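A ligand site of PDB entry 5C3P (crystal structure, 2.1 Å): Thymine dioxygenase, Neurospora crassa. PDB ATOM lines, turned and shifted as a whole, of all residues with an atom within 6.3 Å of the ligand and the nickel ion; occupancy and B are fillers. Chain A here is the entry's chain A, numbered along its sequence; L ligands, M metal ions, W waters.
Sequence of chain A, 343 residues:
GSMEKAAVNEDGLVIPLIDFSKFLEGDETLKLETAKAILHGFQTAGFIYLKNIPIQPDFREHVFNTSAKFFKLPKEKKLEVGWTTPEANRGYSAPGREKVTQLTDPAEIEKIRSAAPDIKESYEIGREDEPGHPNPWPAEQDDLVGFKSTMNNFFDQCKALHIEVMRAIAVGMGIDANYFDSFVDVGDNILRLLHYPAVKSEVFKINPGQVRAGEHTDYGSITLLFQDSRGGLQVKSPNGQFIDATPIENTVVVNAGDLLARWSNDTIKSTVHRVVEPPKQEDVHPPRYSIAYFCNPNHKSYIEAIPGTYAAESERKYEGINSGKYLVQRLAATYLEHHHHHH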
ATOM      1  N   LYS A 120     -22.131  21.291  13.437  1.00  0.00           N
ATOM      2  CA  LYS A 120     -21.953  20.926  14.836  1.00  0.00           C
ATOM      3  C   LYS A 120     -20.765  21.632  15.438  1.00  0.00           C
ATOM      4  O   LYS A 120     -19.888  22.106  14.732  1.00  0.00           O
ATOM      5  CB  LYS A 120     -21.717  19.411  14.962  1.00  0.00           C
ATOM      6  CG  LYS A 120     -20.349  18.948  14.494  1.00  0.00           C
ATOM      7  CD  LYS A 120     -20.128  17.448  14.680  1.00  0.00           C
ATOM      8  CE  LYS A 120     -18.648  17.111  14.639  1.00  0.00           C
ATOM      9  NZ  LYS A 120     -18.397  15.638  14.630  1.00  0.00           N
ATOM     10  N   ARG A 192     -16.808  13.873  25.035  1.00  0.00           N
ATOM     11  CA  ARG A 192     -17.111  14.860  24.003  1.00  0.00           C
ATOM     12  C   ARG A 192     -18.535  15.399  24.116  1.00  0.00           C
ATOM     13  O   ARG A 192     -19.498  14.682  23.834  1.00  0.00           O
ATOM     14  CB  ARG A 192     -16.897  14.275  22.607  1.00  0.00           C
ATOM     15  CG  ARG A 192     -17.144  15.280  21.470  1.00  0.00           C
ATOM     16  CD  ARG A 192     -17.179  14.618  20.103  1.00  0.00           C
ATOM     17  NE  ARG A 192     -15.856  14.343  19.595  1.00  0.00           N
ATOM     18  CZ  ARG A 192     -15.589  13.664  18.478  1.00  0.00           C
ATOM     19  NH1 ARG A 192     -16.577  13.152  17.739  1.00  0.00           N
ATOM     20  NH2 ARG A 192     -14.333  13.473  18.116  1.00  0.00           N
ATOM     21  N   LEU A 194     -21.407  17.553  22.483  1.00  0.00           N
ATOM     22  CA  LEU A 194     -21.773  17.929  21.126  1.00  0.00           C
ATOM     23  C   LEU A 194     -22.992  18.825  21.107  1.00  0.00           C
ATOM     24  O   LEU A 194     -23.949  18.645  21.877  1.00  0.00           O
ATOM     25  CB  LEU A 194     -22.067  16.705  20.270  1.00  0.00           C
ATOM     26  CG  LEU A 194     -20.850  15.841  19.930  1.00  0.00           C
ATOM     27  CD1 LEU A 194     -21.205  14.370  19.816  1.00  0.00           C
ATOM     28  CD2 LEU A 194     -20.190  16.355  18.663  1.00  0.00           C
ATOM     29  N   TYR A 196     -25.464  20.451  18.064  1.00  0.00           N
ATOM     30  CA  TYR A 196     -25.841  20.673  16.681  1.00  0.00           C
ATOM     31  C   TYR A 196     -26.849  21.831  16.658  1.00  0.00           C
ATOM     32  O   TYR A 196     -27.985  21.680  17.126  1.00  0.00           O
ATOM     33  CB  TYR A 196     -26.444  19.397  16.092  1.00  0.00           C
ATOM     34  CG  TYR A 196     -25.559  18.155  16.204  1.00  0.00           C
ATOM     35  CD1 TYR A 196     -25.546  17.383  17.357  1.00  0.00           C
ATOM     36  CD2 TYR A 196     -24.760  17.754  15.131  1.00  0.00           C
ATOM     37  CE1 TYR A 196     -24.745  16.246  17.458  1.00  0.00           C
ATOM     38  CE2 TYR A 196     -23.973  16.603  15.212  1.00  0.00           C
ATOM     39  CZ  TYR A 196     -23.967  15.857  16.370  1.00  0.00           C
ATOM     40  OH  TYR A 196     -23.182  14.711  16.459  1.00  0.00           O
ATOM     41  N   ALA A 213     -23.754  15.012  11.356  1.00  0.00           N
ATOM     42  CA  ALA A 213     -22.468  14.362  11.558  1.00  0.00           C
ATOM     43  C   ALA A 213     -22.259  13.324  10.461  1.00  0.00           C
ATOM     44  O   ALA A 213     -23.115  12.444  10.247  1.00  0.00           O
ATOM     45  CB  ALA A 213     -22.390  13.689  12.916  1.00  0.00           C
ATOM     46  N   HIS A 216     -19.280   7.459   9.684  1.00  0.00           N
ATOM     47  CA  HIS A 216     -17.988   7.046  10.192  1.00  0.00           C
ATOM     48  C   HIS A 216     -18.170   5.857  11.108  1.00  0.00           C
ATOM     49  O   HIS A 216     -19.284   5.505  11.529  1.00  0.00           O
ATOM     50  CB  HIS A 216     -17.325   8.177  11.021  1.00  0.00           C
ATOM     51  CG  HIS A 216     -18.112   8.551  12.229  1.00  0.00           C
ATOM     52  ND1 HIS A 216     -19.268   9.303  12.153  1.00  0.00           N
ATOM     53  CD2 HIS A 216     -17.954   8.256  13.538  1.00  0.00           C
ATOM     54  CE1 HIS A 216     -19.767   9.462  13.363  1.00  0.00           C
ATOM     55  NE2 HIS A 216     -18.985   8.850  14.218  1.00  0.00           N
ATOM     56  N   THR A 217     -17.037   5.235  11.427  1.00  0.00           N
ATOM     57  CA  THR A 217     -16.950   4.337  12.564  1.00  0.00           C
ATOM     58  C   THR A 217     -16.088   5.007  13.616  1.00  0.00           C
ATOM     59  O   THR A 217     -15.190   5.778  13.281  1.00  0.00           O
ATOM     60  CB  THR A 217     -16.308   2.987  12.205  1.00  0.00           C
ATOM     61  OG1 THR A 217     -15.020   3.205  11.619  1.00  0.00           O
ATOM     62  CG2 THR A 217     -17.167   2.218  11.256  1.00  0.00           C
ATOM     63  N   ASP A 218     -16.363   4.726  14.883  1.00  0.00           N
ATOM     64  CA  ASP A 218     -15.526   5.207  15.965  1.00  0.00           C
ATOM     65  C   ASP A 218     -14.229   4.409  16.008  1.00  0.00           C
ATOM     66  O   ASP A 218     -14.202   3.232  15.614  1.00  0.00           O
ATOM     67  CB  ASP A 218     -16.267   5.081  17.309  1.00  0.00           C
ATOM     68  CG  ASP A 218     -17.480   5.987  17.410  1.00  0.00           C
ATOM     69  OD1 ASP A 218     -17.631   6.886  16.563  1.00  0.00           O
ATOM     70  OD2 ASP A 218     -18.284   5.826  18.344  1.00  0.00           O
ATOM     71  N   THR A 223     -17.935   3.272  22.788  1.00  0.00           N
ATOM     72  CA  THR A 223     -18.465   4.628  22.931  1.00  0.00           C
ATOM     73  C   THR A 223     -19.798   4.580  23.663  1.00  0.00           C
ATOM     74  O   THR A 223     -20.680   3.782  23.324  1.00  0.00           O
ATOM     75  CB  THR A 223     -18.659   5.317  21.561  1.00  0.00           C
ATOM     76  OG1 THR A 223     -17.416   5.381  20.900  1.00  0.00           O
ATOM     77  CG2 THR A 223     -19.214   6.725  21.711  1.00  0.00           C
ATOM     78  N   LEU A 225     -22.994   6.719  24.299  1.00  0.00           N
ATOM     79  CA  LEU A 225     -23.645   7.843  23.634  1.00  0.00           C
ATOM     80  C   LEU A 225     -24.950   8.218  24.318  1.00  0.00           C
ATOM     81  O   LEU A 225     -25.920   7.444  24.308  1.00  0.00           O
ATOM     82  CB  LEU A 225     -23.904   7.528  22.148  1.00  0.00           C
ATOM     83  CG  LEU A 225     -24.642   8.645  21.396  1.00  0.00           C
ATOM     84  CD1 LEU A 225     -23.753   9.881  21.222  1.00  0.00           C
ATOM     85  CD2 LEU A 225     -25.111   8.151  20.034  1.00  0.00           C
ATOM     86  N   PHE A 226     -24.963   9.428  24.881  1.00  0.00           N
ATOM     87  CA  PHE A 226     -26.143   9.985  25.512  1.00  0.00           C
ATOM     88  C   PHE A 226     -26.772  10.982  24.539  1.00  0.00           C
ATOM     89  O   PHE A 226     -26.142  11.957  24.165  1.00  0.00           O
ATOM     90  CB  PHE A 226     -25.739  10.689  26.800  1.00  0.00           C
ATOM     91  CG  PHE A 226     -25.024   9.808  27.787  1.00  0.00           C
ATOM     92  CD1 PHE A 226     -23.650   9.582  27.674  1.00  0.00           C
ATOM     93  CD2 PHE A 226     -25.707   9.209  28.829  1.00  0.00           C
ATOM     94  CE1 PHE A 226     -22.982   8.774  28.597  1.00  0.00           C
ATOM     95  CE2 PHE A 226     -25.048   8.398  29.750  1.00  0.00           C
ATOM     96  CZ  PHE A 226     -23.684   8.178  29.630  1.00  0.00           C
ATOM     97  N   GLN A 227     -28.000  10.724  24.112  1.00  0.00           N
ATOM     98  CA  GLN A 227     -28.656  11.660  23.195  1.00  0.00           C
ATOM     99  C   GLN A 227     -29.929  12.244  23.789  1.00  0.00           C
ATOM    100  O   GLN A 227     -30.592  11.608  24.600  1.00  0.00           O
ATOM    101  CB  GLN A 227     -28.922  10.996  21.840  1.00  0.00           C
ATOM    102  CG  GLN A 227     -29.841   9.766  21.888  1.00  0.00           C
ATOM    103  CD  GLN A 227     -30.207   9.252  20.499  1.00  0.00           C
ATOM    104  OE1 GLN A 227     -30.094   9.977  19.506  1.00  0.00           O
ATOM    105  NE2 GLN A 227     -30.665   8.012  20.433  1.00  0.00           N
ATOM    106  N   LEU A 233     -29.766  10.344  14.811  1.00  0.00           N
ATOM    107  CA  LEU A 233     -28.786   9.263  14.773  1.00  0.00           C
ATOM    108  C   LEU A 233     -29.269   8.105  13.897  1.00  0.00           C
ATOM    109  O   LEU A 233     -30.407   7.650  14.017  1.00  0.00           O
ATOM    110  CB  LEU A 233     -28.453   8.759  16.179  1.00  0.00           C
ATOM    111  CG  LEU A 233     -27.396   7.665  16.251  1.00  0.00           C
ATOM    112  CD1 LEU A 233     -26.037   8.168  15.836  1.00  0.00           C
ATOM    113  CD2 LEU A 233     -27.356   7.114  17.665  1.00  0.00           C
ATOM    114  N   ASN A 255     -21.829   1.583  21.521  1.00  0.00           N
ATOM    115  CA  ASN A 255     -21.315   0.938  20.314  1.00  0.00           C
ATOM    116  C   ASN A 255     -19.846   0.626  20.416  1.00  0.00           C
ATOM    117  O   ASN A 255     -19.096   1.317  21.093  1.00  0.00           O
ATOM    118  CB  ASN A 255     -21.569   1.780  19.084  1.00  0.00           C
ATOM    119  CG  ASN A 255     -20.754   3.039  19.057  1.00  0.00           C
ATOM    120  OD1 ASN A 255     -21.021   3.974  19.804  1.00  0.00           O
ATOM    121  ND2 ASN A 255     -19.747   3.097  18.158  1.00  0.00           N
ATOM    122  N   HIS A 273     -22.142   4.735  11.419  1.00  0.00           N
ATOM    123  CA  HIS A 273     -23.282   5.524  11.834  1.00  0.00           C
ATOM    124  C   HIS A 273     -23.051   6.989  11.499  1.00  0.00           C
ATOM    125  O   HIS A 273     -21.914   7.422  11.244  1.00  0.00           O
ATOM    126  CB  HIS A 273     -23.529   5.344  13.329  1.00  0.00           C
ATOM    127  CG  HIS A 273     -22.340   5.617  14.170  1.00  0.00           C
ATOM    128  ND1 HIS A 273     -21.228   4.792  14.181  1.00  0.00           N
ATOM    129  CD2 HIS A 273     -22.058   6.634  15.010  1.00  0.00           C
ATOM    130  CE1 HIS A 273     -20.325   5.291  15.000  1.00  0.00           C
ATOM    131  NE2 HIS A 273     -20.807   6.393  15.526  1.00  0.00           N
ATOM    132  N   ARG A 274     -24.139   7.751  11.551  1.00  0.00           N
ATOM    133  CA  ARG A 274     -24.146   9.171  11.204  1.00  0.00           C
ATOM    134  C   ARG A 274     -25.306   9.862  11.901  1.00  0.00           C
ATOM    135  O   ARG A 274     -26.165   9.213  12.493  1.00  0.00           O
ATOM    136  CB  ARG A 274     -24.288   9.355   9.663  1.00  0.00           C
ATOM    137  CG  ARG A 274     -25.642   8.913   9.129  1.00  0.00           C
ATOM    138  CD  ARG A 274     -25.753   8.999   7.601  1.00  0.00           C
ATOM    139  NE  ARG A 274     -27.133   8.759   7.186  1.00  0.00           N
ATOM    140  CZ  ARG A 274     -27.558   8.761   5.933  1.00  0.00           C
ATOM    141  NH1 ARG A 274     -26.711   9.001   4.948  1.00  0.00           N
ATOM    142  NH2 ARG A 274     -28.845   8.506   5.658  1.00  0.00           N
ATOM    143  N   VAL A 275     -25.320  11.181  11.831  1.00  0.00           N
ATOM    144  CA  VAL A 275     -26.443  11.979  12.308  1.00  0.00           C
ATOM    145  C   VAL A 275     -26.957  12.835  11.168  1.00  0.00           C
ATOM    146  O   VAL A 275     -26.247  13.680  10.633  1.00  0.00           O
ATOM    147  CB  VAL A 275     -26.077  12.891  13.495  1.00  0.00           C
ATOM    148  CG1 VAL A 275     -27.331  13.579  14.026  1.00  0.00           C
ATOM    149  CG2 VAL A 275     -25.408  12.100  14.618  1.00  0.00           C
ATOM    150  N   ARG A 288     -29.866  20.249  18.792  1.00  0.00           N
ATOM    151  CA  ARG A 288     -29.744  18.885  19.291  1.00  0.00           C
ATOM    152  C   ARG A 288     -28.485  18.780  20.106  1.00  0.00           C
ATOM    153  O   ARG A 288     -27.441  19.222  19.664  1.00  0.00           O
ATOM    154  CB  ARG A 288     -29.699  17.872  18.146  1.00  0.00           C
ATOM    155  CG  ARG A 288     -29.278  16.459  18.553  1.00  0.00           C
ATOM    156  CD  ARG A 288     -29.511  15.479  17.406  1.00  0.00           C
ATOM    157  NE  ARG A 288     -29.335  14.099  17.858  1.00  0.00           N
ATOM    158  CZ  ARG A 288     -28.162  13.480  17.964  1.00  0.00           C
ATOM    159  NH1 ARG A 288     -27.026  14.091  17.665  1.00  0.00           N
ATOM    160  NH2 ARG A 288     -28.128  12.228  18.408  1.00  0.00           N
ATOM    161  N   TYR A 289     -28.597  18.206  21.297  1.00  0.00           N
ATOM    162  CA  TYR A 289     -27.465  17.935  22.155  1.00  0.00           C
ATOM    163  C   TYR A 289     -27.250  16.447  22.306  1.00  0.00           C
ATOM    164  O   TYR A 289     -28.212  15.683  22.467  1.00  0.00           O
ATOM    165  CB  TYR A 289     -27.689  18.527  23.545  1.00  0.00           C
ATOM    166  CG  TYR A 289     -27.792  20.023  23.513  1.00  0.00           C
ATOM    167  CD1 TYR A 289     -26.643  20.797  23.621  1.00  0.00           C
ATOM    168  CD2 TYR A 289     -29.008  20.657  23.345  1.00  0.00           C
ATOM    169  CE1 TYR A 289     -26.704  22.166  23.576  1.00  0.00           C
ATOM    170  CE2 TYR A 289     -29.083  22.037  23.301  1.00  0.00           C
ATOM    171  CZ  TYR A 289     -27.919  22.783  23.420  1.00  0.00           C
ATOM    172  OH  TYR A 289     -27.948  24.145  23.378  1.00  0.00           O
ATOM    173  N   SER A 290     -25.985  16.049  22.260  1.00  0.00           N
ATOM    174  CA  SER A 290     -25.587  14.692  22.609  1.00  0.00           C
ATOM    175  C   SER A 290     -24.244  14.770  23.306  1.00  0.00           C
ATOM    176  O   SER A 290     -23.566  15.800  23.285  1.00  0.00           O
ATOM    177  CB  SER A 290     -25.480  13.817  21.356  1.00  0.00           C
ATOM    178  OG  SER A 290     -24.420  14.260  20.545  1.00  0.00           O
ATOM    179  N   ILE A 291     -23.881  13.659  23.942  1.00  0.00           N
ATOM    180  CA  ILE A 291     -22.629  13.524  24.662  1.00  0.00           C
ATOM    181  C   ILE A 291     -22.084  12.130  24.375  1.00  0.00           C
ATOM    182  O   ILE A 291     -22.756  11.138  24.659  1.00  0.00           O
ATOM    183  CB  ILE A 291     -22.817  13.702  26.189  1.00  0.00           C
ATOM    184  CG1 ILE A 291     -23.329  15.116  26.499  1.00  0.00           C
ATOM    185  CG2 ILE A 291     -21.497  13.478  26.930  1.00  0.00           C
ATOM    186  CD1 ILE A 291     -23.717  15.321  27.953  1.00  0.00           C
ATOM    187  N   ALA A 292     -20.898  12.073  23.776  1.00  0.00           N
ATOM    188  CA  ALA A 292     -20.207  10.829  23.475  1.00  0.00           C
ATOM    189  C   ALA A 292     -18.998  10.672  24.396  1.00  0.00           C
ATOM    190  O   ALA A 292     -18.167  11.563  24.507  1.00  0.00           O
ATOM    191  CB  ALA A 292     -19.755  10.795  22.029  1.00  0.00           C
ATOM    192  N   PHE A 294     -15.849   8.472  24.644  1.00  0.00           N
ATOM    193  CA  PHE A 294     -15.038   7.540  23.878  1.00  0.00           C
ATOM    194  C   PHE A 294     -14.095   6.836  24.824  1.00  0.00           C
ATOM    195  O   PHE A 294     -13.221   7.487  25.444  1.00  0.00           O
ATOM    196  CB  PHE A 294     -14.260   8.270  22.781  1.00  0.00           C
ATOM    197  CG  PHE A 294     -15.140   8.969  21.785  1.00  0.00           C
ATOM    198  CD1 PHE A 294     -15.780   8.244  20.780  1.00  0.00           C
ATOM    199  CD2 PHE A 294     -15.326  10.339  21.847  1.00  0.00           C
ATOM    200  CE1 PHE A 294     -16.591   8.896  19.864  1.00  0.00           C
ATOM    201  CE2 PHE A 294     -16.127  10.993  20.932  1.00  0.00           C
ATOM    202  CZ  PHE A 294     -16.770  10.274  19.935  1.00  0.00           C
HETATM  203  C1  LIG L   1     -19.473  10.827  17.316  1.00  0.00           C
HETATM  204  O1  LIG L   1     -18.608   9.936  17.163  1.00  0.00           O
HETATM  205  O2  LIG L   1     -19.170  11.988  17.694  1.00  0.00           O
HETATM  206  C2  LIG L   1     -20.886  10.490  17.029  1.00  0.00           C
HETATM  207  O3  LIG L   1     -21.155   9.449  16.433  1.00  0.00           O
HETATM  208  C3  LIG L   1     -21.983  11.443  17.462  1.00  0.00           C
HETATM  209  C4  LIG L   1     -23.349  10.777  17.434  1.00  0.00           C
HETATM  210  C5  LIG L   1     -24.436  11.646  18.025  1.00  0.00           C
HETATM  211  O4  LIG L   1     -25.521  11.095  18.315  1.00  0.00           O
HETATM  212  O5  LIG L   1     -24.252  12.873  18.181  1.00  0.00           O
HETATM  213 NI    NI M   1     -19.526   8.036  16.336  1.00  0.00          NI
HETATM  214  O   HOH W   1     -20.175   7.536  18.482  1.00  0.00           O
HETATM  215  O   HOH W   2     -16.094  10.199  16.260  1.00  0.00           O
HETATM  216  O   HOH W   3     -20.012  14.312  15.917  1.00  0.00           O
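An oxygen (O5) of the ligand lies within hydrogen-bond range of the side-chain hydroxyl of Tyr 196 (2.7 Å). The side-chain hydroxyl (OG) of Ser 290 sits at hydrogen-bond distance from an oxygen (O5) of the ligand (2.7 Å). The guanidinium group (NH1) of Arg 192 lies within salt-bridge range of an oxygen (O2) of the ligand (2.8 Å). The guanidinium group (NH2) of Arg 288 is in salt-bridge range of an oxygen (O4) of the ligand (2.8 Å).
The side-chain amide nitrogen of Asn 255 is in hydrogen-bond range of the side-chain carboxylate of Asp 218. The side-chain hydroxyl of Thr 223 lies within hydrogen-bond range of the side-chain carboxylate of Asp 218 (2.7 Å). N of Tyr 196 sits at hydrogen-bond distance from O of Arg 288 (2.8 Å). The backbone carbonyl oxygen (O) of Ser 290 sits at hydrogen-bond distance from the backbone NH (N) of Leu 194 (2.9 Å). N of Arg 192 sits at hydrogen-bond distance from O of Ala 292, at 2.7 Å. The side-chain amide oxygen of Gln 227 sits at hydrogen-bond distance from the guanidinium group of Arg 288 (3.2 Å). O of Val 275 is in hydrogen-bond range of N of Ala 213, 2.9 Å away.
Residues that only touch the ligand: Leu 194 (3.8 Å), Leu 225 (3.4 Å), Leu 233 (3.9 Å), Val 275 (3.6 Å) and Phe 294 (3.3 Å). Hydrophobic or aromatic side chains within 4 Å of the ligand: Leu 194, Tyr 196, His 216, Leu 225, Leu 233, His 273, Val 275 and Phe 294. Within 4 Å of the ligand: Arg 192, Leu 194, Tyr 196, His 216, Asp 218, Leu 225, Leu 233, His 273, Val 275, Arg 288, Ser 290 and Phe 294. Along chain A the residues within 4 Å of the ligand span positions 192 to 294.
Of the 23 residues printed, 3 come within 4 Å of the nickel ion. The nearest printed residue that does not touch the nickel ion is Phe 294 (4.7 Å).
The nickel ion is bound by O3 of the ligand (2.2 Å). OD1 of Asp 218 is bound to the nickel ion. NE2 of His 273 is bound to the nickel ion, 2.2 Å away. O1 of the ligand binds the nickel ion (2.3 Å). Water W1 is bound to the nickel ion, 2.3 Å away. The nickel ion is bound by NE2 of His 216.
Water W3 lies within hydrogen-bond range of the side-chain amino group (NZ) of Lys 120 (2.5 Å), an oxygen (O2) of the ligand (3.0 Å) and the side-chain hydroxyl (OH) of Tyr 196 (3.2 Å).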
